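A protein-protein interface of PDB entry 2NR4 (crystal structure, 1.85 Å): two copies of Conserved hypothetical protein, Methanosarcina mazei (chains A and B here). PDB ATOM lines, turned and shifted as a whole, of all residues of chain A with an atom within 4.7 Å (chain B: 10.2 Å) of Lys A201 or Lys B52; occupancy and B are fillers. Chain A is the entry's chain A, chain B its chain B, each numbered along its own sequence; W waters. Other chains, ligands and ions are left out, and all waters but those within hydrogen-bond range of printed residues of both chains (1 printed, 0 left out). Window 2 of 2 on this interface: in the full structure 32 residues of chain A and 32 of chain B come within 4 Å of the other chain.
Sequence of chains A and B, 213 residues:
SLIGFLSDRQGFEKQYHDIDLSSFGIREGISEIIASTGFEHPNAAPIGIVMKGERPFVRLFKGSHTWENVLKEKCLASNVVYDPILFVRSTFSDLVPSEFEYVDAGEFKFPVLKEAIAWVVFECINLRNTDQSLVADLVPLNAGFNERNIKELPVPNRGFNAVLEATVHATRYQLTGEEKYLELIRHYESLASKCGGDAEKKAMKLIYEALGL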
ATOM      1  N   ALA A 192      31.659  -3.372  15.368  1.00  0.00           N
ATOM      2  CA  ALA A 192      30.378  -4.020  15.296  1.00  0.00           C
ATOM      3  C   ALA A 192      30.542  -5.523  15.508  1.00  0.00           C
ATOM      4  O   ALA A 192      29.697  -6.170  16.131  1.00  0.00           O
ATOM      5  CB  ALA A 192      29.733  -3.751  13.911  1.00  0.00           C
ATOM      6  N   SER A 193      31.620  -6.059  14.931  1.00  0.00           N
ATOM      7  CA  SER A 193      31.945  -7.464  15.072  1.00  0.00           C
ATOM      8  C   SER A 193      32.330  -7.846  16.504  1.00  0.00           C
ATOM      9  O   SER A 193      31.971  -8.936  16.960  1.00  0.00           O
ATOM     10  CB  SER A 193      33.092  -7.851  14.151  1.00  0.00           C
ATOM     11  OG  SER A 193      33.065  -9.273  14.052  1.00  0.00           O
ATOM     12  N   LYS A 194      33.095  -6.976  17.177  1.00  0.00           N
ATOM     13  CA  LYS A 194      33.551  -7.246  18.542  1.00  0.00           C
ATOM     14  C   LYS A 194      32.444  -7.021  19.535  1.00  0.00           C
ATOM     15  O   LYS A 194      32.211  -7.861  20.412  1.00  0.00           O
ATOM     16  CB  LYS A 194      34.758  -6.383  18.905  1.00  0.00           C
ATOM     17  CG  LYS A 194      35.936  -6.611  17.995  1.00  0.00           C
ATOM     18  CD  LYS A 194      37.105  -5.673  18.325  1.00  0.00           C
ATOM     19  CE  LYS A 194      38.445  -6.311  17.910  1.00  0.00           C
ATOM     20  NZ  LYS A 194      38.608  -7.646  18.595  1.00  0.00           N
ATOM     21  N   GLY A 196      28.978  -5.838  18.820  1.00  0.00           N
ATOM     22  CA  GLY A 196      27.563  -5.999  18.489  1.00  0.00           C
ATOM     23  C   GLY A 196      27.105  -7.423  18.676  1.00  0.00           C
ATOM     24  O   GLY A 196      27.930  -8.307  18.903  1.00  0.00           O
ATOM     25  N   GLY A 197      25.807  -7.615  18.613  1.00  0.00           N
ATOM     26  CA  GLY A 197      25.178  -8.917  18.439  1.00  0.00           C
ATOM     27  C   GLY A 197      24.953  -9.238  16.985  1.00  0.00           C
ATOM     28  O   GLY A 197      25.487  -8.543  16.086  1.00  0.00           O
ATOM     29  N   ASP A 198      24.157 -10.290  16.754  1.00  0.00           N
ATOM     30  CA  ASP A 198      23.742 -10.686  15.396  1.00  0.00           C
ATOM     31  C   ASP A 198      23.125  -9.551  14.570  1.00  0.00           C
ATOM     32  O   ASP A 198      23.416  -9.434  13.377  1.00  0.00           O
ATOM     33  CB  ASP A 198      22.754 -11.862  15.434  1.00  0.00           C
ATOM     34  CG  ASP A 198      23.420 -13.171  15.807  1.00  0.00           C
ATOM     35  OD1 ASP A 198      24.664 -13.212  15.771  1.00  0.00           O
ATOM     36  OD2 ASP A 198      22.710 -14.154  16.142  1.00  0.00           O
ATOM     37  N   ALA A 199      22.259  -8.735  15.176  1.00  0.00           N
ATOM     38  CA  ALA A 199      21.597  -7.657  14.434  1.00  0.00           C
ATOM     39  C   ALA A 199      22.597  -6.634  13.888  1.00  0.00           C
ATOM     40  O   ALA A 199      22.508  -6.233  12.716  1.00  0.00           O
ATOM     41  CB  ALA A 199      20.542  -6.967  15.292  1.00  0.00           C
ATOM     42  N   GLU A 200      23.558  -6.220  14.725  1.00  0.00           N
ATOM     43  CA  GLU A 200      24.623  -5.334  14.250  1.00  0.00           C
ATOM     44  C   GLU A 200      25.473  -5.921  13.137  1.00  0.00           C
ATOM     45  O   GLU A 200      25.854  -5.231  12.175  1.00  0.00           O
ATOM     46  CB  GLU A 200      25.532  -4.883  15.397  1.00  0.00           C
ATOM     47  CG  GLU A 200      24.875  -3.882  16.326  1.00  0.00           C
ATOM     48  CD  GLU A 200      23.896  -4.489  17.292  1.00  0.00           C
ATOM     49  OE1 GLU A 200      24.030  -5.700  17.601  1.00  0.00           O
ATOM     50  OE2 GLU A 200      22.980  -3.747  17.748  1.00  0.00           O
ATOM     51  N   LYS A 201      25.794  -7.204  13.271  1.00  0.00           N
ATOM     52  CA  LYS A 201      26.635  -7.835  12.271  1.00  0.00           C
ATOM     53  C   LYS A 201      25.891  -7.935  10.937  1.00  0.00           C
ATOM     54  O   LYS A 201      26.493  -7.681   9.897  1.00  0.00           O
ATOM     55  CB  LYS A 201      27.210  -9.164  12.780  1.00  0.00           C
ATOM     56  CG  LYS A 201      28.181  -8.987  13.981  1.00  0.00           C
ATOM     57  CD  LYS A 201      28.578 -10.379  14.553  1.00  0.00           C
ATOM     58  CE  LYS A 201      29.278 -10.277  15.907  1.00  0.00           C
ATOM     59  NZ  LYS A 201      29.449 -11.635  16.534  1.00  0.00           N
ATOM     60  N   LYS A 202      24.592  -8.215  10.986  1.00  0.00           N
ATOM     61  CA  LYS A 202      23.710  -8.176   9.802  1.00  0.00           C
ATOM     62  C   LYS A 202      23.599  -6.767   9.199  1.00  0.00           C
ATOM     63  O   LYS A 202      23.631  -6.599   7.973  1.00  0.00           O
ATOM     64  CB  LYS A 202      22.296  -8.693  10.132  1.00  0.00           C
ATOM     65  CG  LYS A 202      22.148 -10.201  10.289  1.00  0.00           C
ATOM     66  CD  LYS A 202      20.666 -10.639  10.130  1.00  0.00           C
ATOM     67  CE  LYS A 202      20.271 -11.663  11.227  1.00  0.00           C
ATOM     68  NZ  LYS A 202      21.353 -12.688  11.408  1.00  0.00           N
ATOM     69  N   ALA A 203      23.489  -5.752  10.069  1.00  0.00           N
ATOM     70  CA  ALA A 203      23.431  -4.351   9.628  1.00  0.00           C
ATOM     71  C   ALA A 203      24.671  -3.922   8.858  1.00  0.00           C
ATOM     72  O   ALA A 203      24.566  -3.311   7.801  1.00  0.00           O
ATOM     73  CB  ALA A 203      23.177  -3.409  10.817  1.00  0.00           C
ATOM     74  N   MET A 204      25.847  -4.283   9.366  1.00  0.00           N
ATOM     75  CA  MET A 204      27.090  -3.978   8.673  1.00  0.00           C
ATOM     76  C   MET A 204      27.137  -4.629   7.307  1.00  0.00           C
ATOM     77  O   MET A 204      27.562  -4.001   6.345  1.00  0.00           O
ATOM     78  CB  MET A 204      28.304  -4.420   9.495  1.00  0.00           C
ATOM     79  CG  MET A 204      28.669  -3.476  10.622  1.00  0.00           C
ATOM     80  SD  MET A 204      28.880  -1.722  10.178  1.00  0.00           S
ATOM     81  CE  MET A 204      30.092  -1.747   8.985  1.00  0.00           C
ATOM     82  N   LYS A 205      26.691  -5.874   7.208  1.00  0.00           N
ATOM     83  CA  LYS A 205      26.637  -6.569   5.917  1.00  0.00           C
ATOM     84  C   LYS A 205      25.762  -5.796   4.925  1.00  0.00           C
ATOM     85  O   LYS A 205      26.110  -5.659   3.742  1.00  0.00           O
ATOM     86  CB  LYS A 205      26.104  -7.988   6.102  1.00  0.00           C
ATOM     87  CG  LYS A 205      26.925  -9.097   5.385  1.00  0.00           C
ATOM     88  CD  LYS A 205      26.430 -10.507   5.779  1.00  0.00           C
ATOM     89  CE  LYS A 205      27.590 -11.508   5.986  1.00  0.00           C
ATOM     90  NZ  LYS A 205      27.817 -12.531   4.892  1.00  0.00           N
ATOM     91  N   LEU B  21      18.376 -12.016  32.007  1.00  0.00           N
ATOM     92  CA  LEU B  21      19.372 -10.950  32.050  1.00  0.00           C
ATOM     93  C   LEU B  21      19.023  -9.804  31.092  1.00  0.00           C
ATOM     94  O   LEU B  21      19.254  -8.645  31.420  1.00  0.00           O
ATOM     95  CB  LEU B  21      20.768 -11.511  31.769  1.00  0.00           C
ATOM     96  CG  LEU B  21      21.276 -12.495  32.837  1.00  0.00           C
ATOM     97  CD1 LEU B  21      22.576 -13.105  32.402  1.00  0.00           C
ATOM     98  CD2 LEU B  21      21.456 -11.814  34.202  1.00  0.00           C
ATOM     99  N   ILE B  26      21.611  -6.804  30.283  1.00  0.00           N
ATOM    100  CA  ILE B  26      22.743  -7.676  29.955  1.00  0.00           C
ATOM    101  C   ILE B  26      22.380  -8.458  28.713  1.00  0.00           C
ATOM    102  O   ILE B  26      21.672  -9.459  28.772  1.00  0.00           O
ATOM    103  CB  ILE B  26      23.175  -8.631  31.109  1.00  0.00           C
ATOM    104  CG1 ILE B  26      23.425  -7.825  32.393  1.00  0.00           C
ATOM    105  CG2 ILE B  26      24.418  -9.412  30.714  1.00  0.00           C
ATOM    106  CD1 ILE B  26      24.303  -6.609  32.185  1.00  0.00           C
ATOM    107  N   ARG B  27      22.874  -7.972  27.585  1.00  0.00           N
ATOM    108  CA  ARG B  27      22.315  -8.392  26.310  1.00  0.00           C
ATOM    109  C   ARG B  27      23.366  -8.928  25.393  1.00  0.00           C
ATOM    110  O   ARG B  27      24.546  -8.799  25.653  1.00  0.00           O
ATOM    111  CB  ARG B  27      21.537  -7.232  25.709  1.00  0.00           C
ATOM    112  CG  ARG B  27      20.249  -6.963  26.519  1.00  0.00           C
ATOM    113  CD  ARG B  27      19.509  -5.825  25.989  1.00  0.00           C
ATOM    114  NE  ARG B  27      19.180  -6.025  24.569  1.00  0.00           N
ATOM    115  CZ  ARG B  27      18.608  -5.091  23.825  1.00  0.00           C
ATOM    116  NH1 ARG B  27      18.299  -3.935  24.397  1.00  0.00           N
ATOM    117  NH2 ARG B  27      18.331  -5.314  22.534  1.00  0.00           N
ATOM    118  N   GLU B  28      22.922  -9.557  24.304  1.00  0.00           N
ATOM    119  CA  GLU B  28      23.835 -10.085  23.322  1.00  0.00           C
ATOM    120  C   GLU B  28      24.883  -9.035  22.958  1.00  0.00           C
ATOM    121  O   GLU B  28      24.532  -7.858  22.788  1.00  0.00           O
ATOM    122  CB  GLU B  28      23.027 -10.475  22.085  1.00  0.00           C
ATOM    123  CG  GLU B  28      23.838 -11.170  21.004  1.00  0.00           C
ATOM    124  CD  GLU B  28      23.046 -11.371  19.700  1.00  0.00           C
ATOM    125  OE1 GLU B  28      21.827 -11.051  19.646  1.00  0.00           O
ATOM    126  OE2 GLU B  28      23.655 -11.848  18.716  1.00  0.00           O
ATOM    127  N   GLY B  29      26.146  -9.461  22.860  1.00  0.00           N
ATOM    128  CA  GLY B  29      27.265  -8.624  22.459  1.00  0.00           C
ATOM    129  C   GLY B  29      27.927  -8.070  23.711  1.00  0.00           C
ATOM    130  O   GLY B  29      27.866  -8.714  24.765  1.00  0.00           O
ATOM    131  N   ILE B  30      28.508  -6.874  23.615  1.00  0.00           N
ATOM    132  CA  ILE B  30      29.155  -6.256  24.798  1.00  0.00           C
ATOM    133  C   ILE B  30      28.284  -5.108  25.321  1.00  0.00           C
ATOM    134  O   ILE B  30      28.122  -4.105  24.625  1.00  0.00           O
ATOM    135  CB  ILE B  30      30.580  -5.828  24.512  1.00  0.00           C
ATOM    136  CG1 ILE B  30      31.414  -7.040  24.012  1.00  0.00           C
ATOM    137  CG2 ILE B  30      31.208  -5.142  25.764  1.00  0.00           C
ATOM    138  CD1 ILE B  30      32.876  -6.728  23.719  1.00  0.00           C
ATOM    139  N   SER B  31      27.723  -5.265  26.537  1.00  0.00           N
ATOM    140  CA  SER B  31      26.832  -4.260  27.117  1.00  0.00           C
ATOM    141  C   SER B  31      27.709  -3.344  27.979  1.00  0.00           C
ATOM    142  O   SER B  31      28.410  -3.833  28.872  1.00  0.00           O
ATOM    143  CB  SER B  31      25.775  -4.925  28.000  1.00  0.00           C
ATOM    144  OG  SER B  31      25.116  -5.975  27.300  1.00  0.00           O
ATOM    145  N   ILE B  49      30.308  -6.034  29.754  1.00  0.00           N
ATOM    146  CA  ILE B  49      29.962  -7.433  30.025  1.00  0.00           C
ATOM    147  C   ILE B  49      29.650  -8.104  28.671  1.00  0.00           C
ATOM    148  O   ILE B  49      28.848  -7.578  27.883  1.00  0.00           O
ATOM    149  CB  ILE B  49      28.803  -7.491  30.964  1.00  0.00           C
ATOM    150  CG1 ILE B  49      29.261  -6.880  32.319  1.00  0.00           C
ATOM    151  CG2 ILE B  49      28.208  -8.953  31.045  1.00  0.00           C
ATOM    152  CD1 ILE B  49      28.423  -7.265  33.454  1.00  0.00           C
ATOM    153  N   VAL B  50      30.303  -9.232  28.407  1.00  0.00           N
ATOM    154  CA  VAL B  50      30.211  -9.878  27.091  1.00  0.00           C
ATOM    155  C   VAL B  50      29.249 -11.044  27.126  1.00  0.00           C
ATOM    156  O   VAL B  50      29.331 -11.916  28.016  1.00  0.00           O
ATOM    157  CB  VAL B  50      31.572 -10.391  26.591  1.00  0.00           C
ATOM    158  CG1 VAL B  50      31.480 -10.780  25.087  1.00  0.00           C
ATOM    159  CG2 VAL B  50      32.685  -9.397  26.855  1.00  0.00           C
ATOM    160  N   MET B  51      28.345 -11.093  26.154  1.00  0.00           N
ATOM    161  CA  MET B  51      27.440 -12.222  26.080  1.00  0.00           C
ATOM    162  C   MET B  51      27.521 -12.769  24.659  1.00  0.00           C
ATOM    163  O   MET B  51      27.136 -12.075  23.718  1.00  0.00           O
ATOM    164  CB  MET B  51      26.028 -11.766  26.415  1.00  0.00           C
ATOM    165  CG  MET B  51      24.973 -12.831  26.271  1.00  0.00           C
ATOM    166  SD  MET B  51      24.769 -13.609  27.886  1.00  0.00           S
ATOM    167  CE  MET B  51      23.794 -12.316  28.629  1.00  0.00           C
ATOM    168  N   LYS B  52      28.070 -13.977  24.512  1.00  0.00           N
ATOM    169  CA  LYS B  52      28.229 -14.582  23.188  1.00  0.00           C
ATOM    170  C   LYS B  52      27.627 -15.979  23.155  1.00  0.00           C
ATOM    171  O   LYS B  52      28.262 -16.891  22.683  1.00  0.00           O
ATOM    172  CB  LYS B  52      29.708 -14.631  22.765  1.00  0.00           C
ATOM    173  CG  LYS B  52      30.470 -13.287  22.549  1.00  0.00           C
ATOM    174  CD  LYS B  52      29.831 -12.364  21.522  1.00  0.00           C
ATOM    175  CE  LYS B  52      30.815 -11.299  20.999  1.00  0.00           C
ATOM    176  NZ  LYS B  52      30.154 -10.405  19.965  1.00  0.00           N
ATOM    177  N   GLY B  53      26.416 -16.154  23.670  1.00  0.00           N
ATOM    178  CA  GLY B  53      25.743 -17.446  23.579  1.00  0.00           C
ATOM    179  C   GLY B  53      25.748 -18.293  24.848  1.00  0.00           C
ATOM    180  O   GLY B  53      24.778 -19.015  25.121  1.00  0.00           O
ATOM    181  N   GLU B  54      26.817 -18.201  25.633  1.00  0.00           N
ATOM    182  CA  GLU B  54      26.911 -18.959  26.898  1.00  0.00           C
ATOM    183  C   GLU B  54      26.713 -18.031  28.107  1.00  0.00           C
ATOM    184  O   GLU B  54      25.912 -17.099  28.036  1.00  0.00           O
ATOM    185  CB  GLU B  54      28.249 -19.698  26.971  1.00  0.00           C
ATOM    186  CG  GLU B  54      29.471 -18.819  26.756  1.00  0.00           C
ATOM    187  CD  GLU B  54      30.777 -19.600  26.765  1.00  0.00           C
ATOM    188  OE1 GLU B  54      30.745 -20.796  26.349  1.00  0.00           O
ATOM    189  OE2 GLU B  54      31.823 -19.015  27.186  1.00  0.00           O
ATOM    190  N   ARG B  55      27.425 -18.283  29.212  1.00  0.00           N
ATOM    191  CA  ARG B  55      27.362 -17.384  30.362  1.00  0.00           C
ATOM    192  C   ARG B  55      27.960 -16.031  30.007  1.00  0.00           C
ATOM    193  O   ARG B  55      28.924 -15.944  29.221  1.00  0.00           O
ATOM    194  CB  ARG B  55      28.085 -17.960  31.596  1.00  0.00           C
ATOM    195  CG  ARG B  55      27.370 -19.172  32.198  1.00  0.00           C
ATOM    196  CD  ARG B  55      28.053 -19.669  33.493  1.00  0.00           C
ATOM    197  NE  ARG B  55      27.452 -20.922  33.978  1.00  0.00           N
ATOM    198  CZ  ARG B  55      26.311 -20.997  34.659  1.00  0.00           C
ATOM    199  NH1 ARG B  55      25.620 -19.901  34.939  1.00  0.00           N
ATOM    200  NH2 ARG B  55      25.841 -22.173  35.064  1.00  0.00           N
ATOM    201  N   PRO B  56      27.415 -14.967  30.606  1.00  0.00           N
ATOM    202  CA  PRO B  56      28.103 -13.690  30.386  1.00  0.00           C
ATOM    203  C   PRO B  56      29.511 -13.759  30.959  1.00  0.00           C
ATOM    204  O   PRO B  56      29.756 -14.565  31.901  1.00  0.00           O
ATOM    205  CB  PRO B  56      27.259 -12.670  31.174  1.00  0.00           C
ATOM    206  CG  PRO B  56      26.288 -13.436  31.995  1.00  0.00           C
ATOM    207  CD  PRO B  56      26.207 -14.839  31.442  1.00  0.00           C
ATOM    208  N   PHE B  57      30.427 -12.961  30.425  1.00  0.00           N
ATOM    209  CA  PHE B  57      31.772 -12.892  30.989  1.00  0.00           C
ATOM    210  C   PHE B  57      32.403 -11.475  30.954  1.00  0.00           C
ATOM    211  O   PHE B  57      31.902 -10.590  30.245  1.00  0.00           O
ATOM    212  CB  PHE B  57      32.717 -13.950  30.399  1.00  0.00           C
ATOM    213  CG  PHE B  57      33.122 -13.691  28.981  1.00  0.00           C
ATOM    214  CD1 PHE B  57      34.290 -13.028  28.702  1.00  0.00           C
ATOM    215  CD2 PHE B  57      32.318 -14.114  27.934  1.00  0.00           C
ATOM    216  CE1 PHE B  57      34.680 -12.782  27.391  1.00  0.00           C
ATOM    217  CE2 PHE B  57      32.712 -13.885  26.605  1.00  0.00           C
ATOM    218  CZ  PHE B  57      33.868 -13.213  26.351  1.00  0.00           C
ATOM    219  N   VAL B  58      33.473 -11.265  31.722  1.00  0.00           N
ATOM    220  CA  VAL B  58      34.195  -9.991  31.710  1.00  0.00           C
ATOM    221  C   VAL B  58      35.663 -10.180  31.411  1.00  0.00           C
ATOM    222  O   VAL B  58      36.260 -11.211  31.783  1.00  0.00           O
ATOM    223  CB  VAL B  58      34.067  -9.178  33.048  1.00  0.00           C
ATOM    224  CG1 VAL B  58      32.699  -8.585  33.172  1.00  0.00           C
ATOM    225  CG2 VAL B  58      34.427 -10.036  34.263  1.00  0.00           C
ATOM    226  N   ARG B  59      36.250  -9.199  30.725  1.00  0.00           N
ATOM    227  CA  ARG B  59      37.670  -9.187  30.518  1.00  0.00           C
ATOM    228  C   ARG B  59      38.210  -7.941  31.162  1.00  0.00           C
ATOM    229  O   ARG B  59      37.981  -6.813  30.687  1.00  0.00           O
ATOM    230  CB  ARG B  59      38.030  -9.227  29.020  1.00  0.00           C
ATOM    231  CG  ARG B  59      39.530  -9.379  28.755  1.00  0.00           C
ATOM    232  CD  ARG B  59      39.820  -9.642  27.263  1.00  0.00           C
ATOM    233  NE  ARG B  59      38.889 -10.618  26.664  1.00  0.00           N
ATOM    234  CZ  ARG B  59      39.195 -11.893  26.394  1.00  0.00           C
ATOM    235  NH1 ARG B  59      40.405 -12.356  26.678  1.00  0.00           N
ATOM    236  NH2 ARG B  59      38.292 -12.702  25.839  1.00  0.00           N
ATOM    237  N   ASP B 137      33.866 -15.732  34.003  1.00  0.00           N
ATOM    238  CA  ASP B 137      32.446 -15.919  33.715  1.00  0.00           C
ATOM    239  C   ASP B 137      31.604 -15.430  34.881  1.00  0.00           C
ATOM    240  O   ASP B 137      32.103 -15.327  36.013  1.00  0.00           O
ATOM    241  CB  ASP B 137      32.124 -17.392  33.409  1.00  0.00           C
ATOM    242  CG  ASP B 137      32.984 -17.940  32.304  1.00  0.00           C
ATOM    243  OD1 ASP B 137      33.103 -17.277  31.247  1.00  0.00           O
ATOM    244  OD2 ASP B 137      33.599 -19.018  32.501  1.00  0.00           O
HETATM  245  O   HOH W   1      21.217  -9.126  17.758  1.00  0.00           O
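Water W1 lies within hydrogen-bond range of the side-chain carboxylate (OE1) of Glu B28 (2.8 Å), the backbone NH (N) of Ala A199 (2.8 Å) and the backbone NH (N) of Asp A198 (3.3 Å).
No position is printed for both chains. Of the 8 pairs that touch across the chains among the printed residues, none has its exchanged pair printed and touching as well.
Lys B52 touches Ser A193 (NZ to O, 3.8 Å). O of Lys A194 touches CD1 of Ile B30, 3.6 Å away. CA of Gly B29 touches O of Gly A196 (3.6 Å). Gly A197 touches Glu B28 (CA to OE2, 3.3 Å). NZ of Lys A201 touches NZ of Lys B52, at 3.7 Å.
OE2 of Glu B28 is in hydrogen-bond range of N of Asp A198 (2.6 Å). NZ of Lys B52 is in hydrogen-bond range of O of Gly A196, at 3.2 Å. NZ of Lys B52 is in hydrogen-bond range of O of Lys A194 (3.3 Å).
Of chain B, only Lys B52 (3.8 Å) comes within 4 Å of Ser A193. Of the printed residues of chain B, Lys A194 touches Ile B30 (3.6 Å) and Lys B52 (3.3 Å). Of chain B, only Gly B29 (3.6 Å) and Lys B52 (3.2 Å) come within 4 Å of Gly A196. No residue of chain B comes within 4 Å of Ala A199. Printed residues of chain B within 4 Å of Lys A201: Lys B52 (3.7 Å). Printed residues of chain A within 4 Å of Gly B29: Gly A196. Lys B52 touches four residues of chain A. Arg B59 touches none of the printed residues of chain A. The nearest residue of chain B that does not touch Lys A201 is Glu B28 (6.2 Å).
The backbone NH (N) of Gly A197 sits at hydrogen-bond distance from the side-chain carboxylate (OE1) of Glu A200 (2.8 Å). The backbone carbonyl oxygen (O) of Gly B29 sits at hydrogen-bond distance from the backbone NH (N) of Met B51, at 2.8 Å.
Printed residues of chain B that touch a printed residue of chain A: Glu B28, Gly B29, Ile B30 and Lys B52. Hydrophobic or aromatic side chains of chain B that line the printed part of chain A: Ile B30. Along chain B the printed residues that touch a printed residue of chain A span positions 28 to 52.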
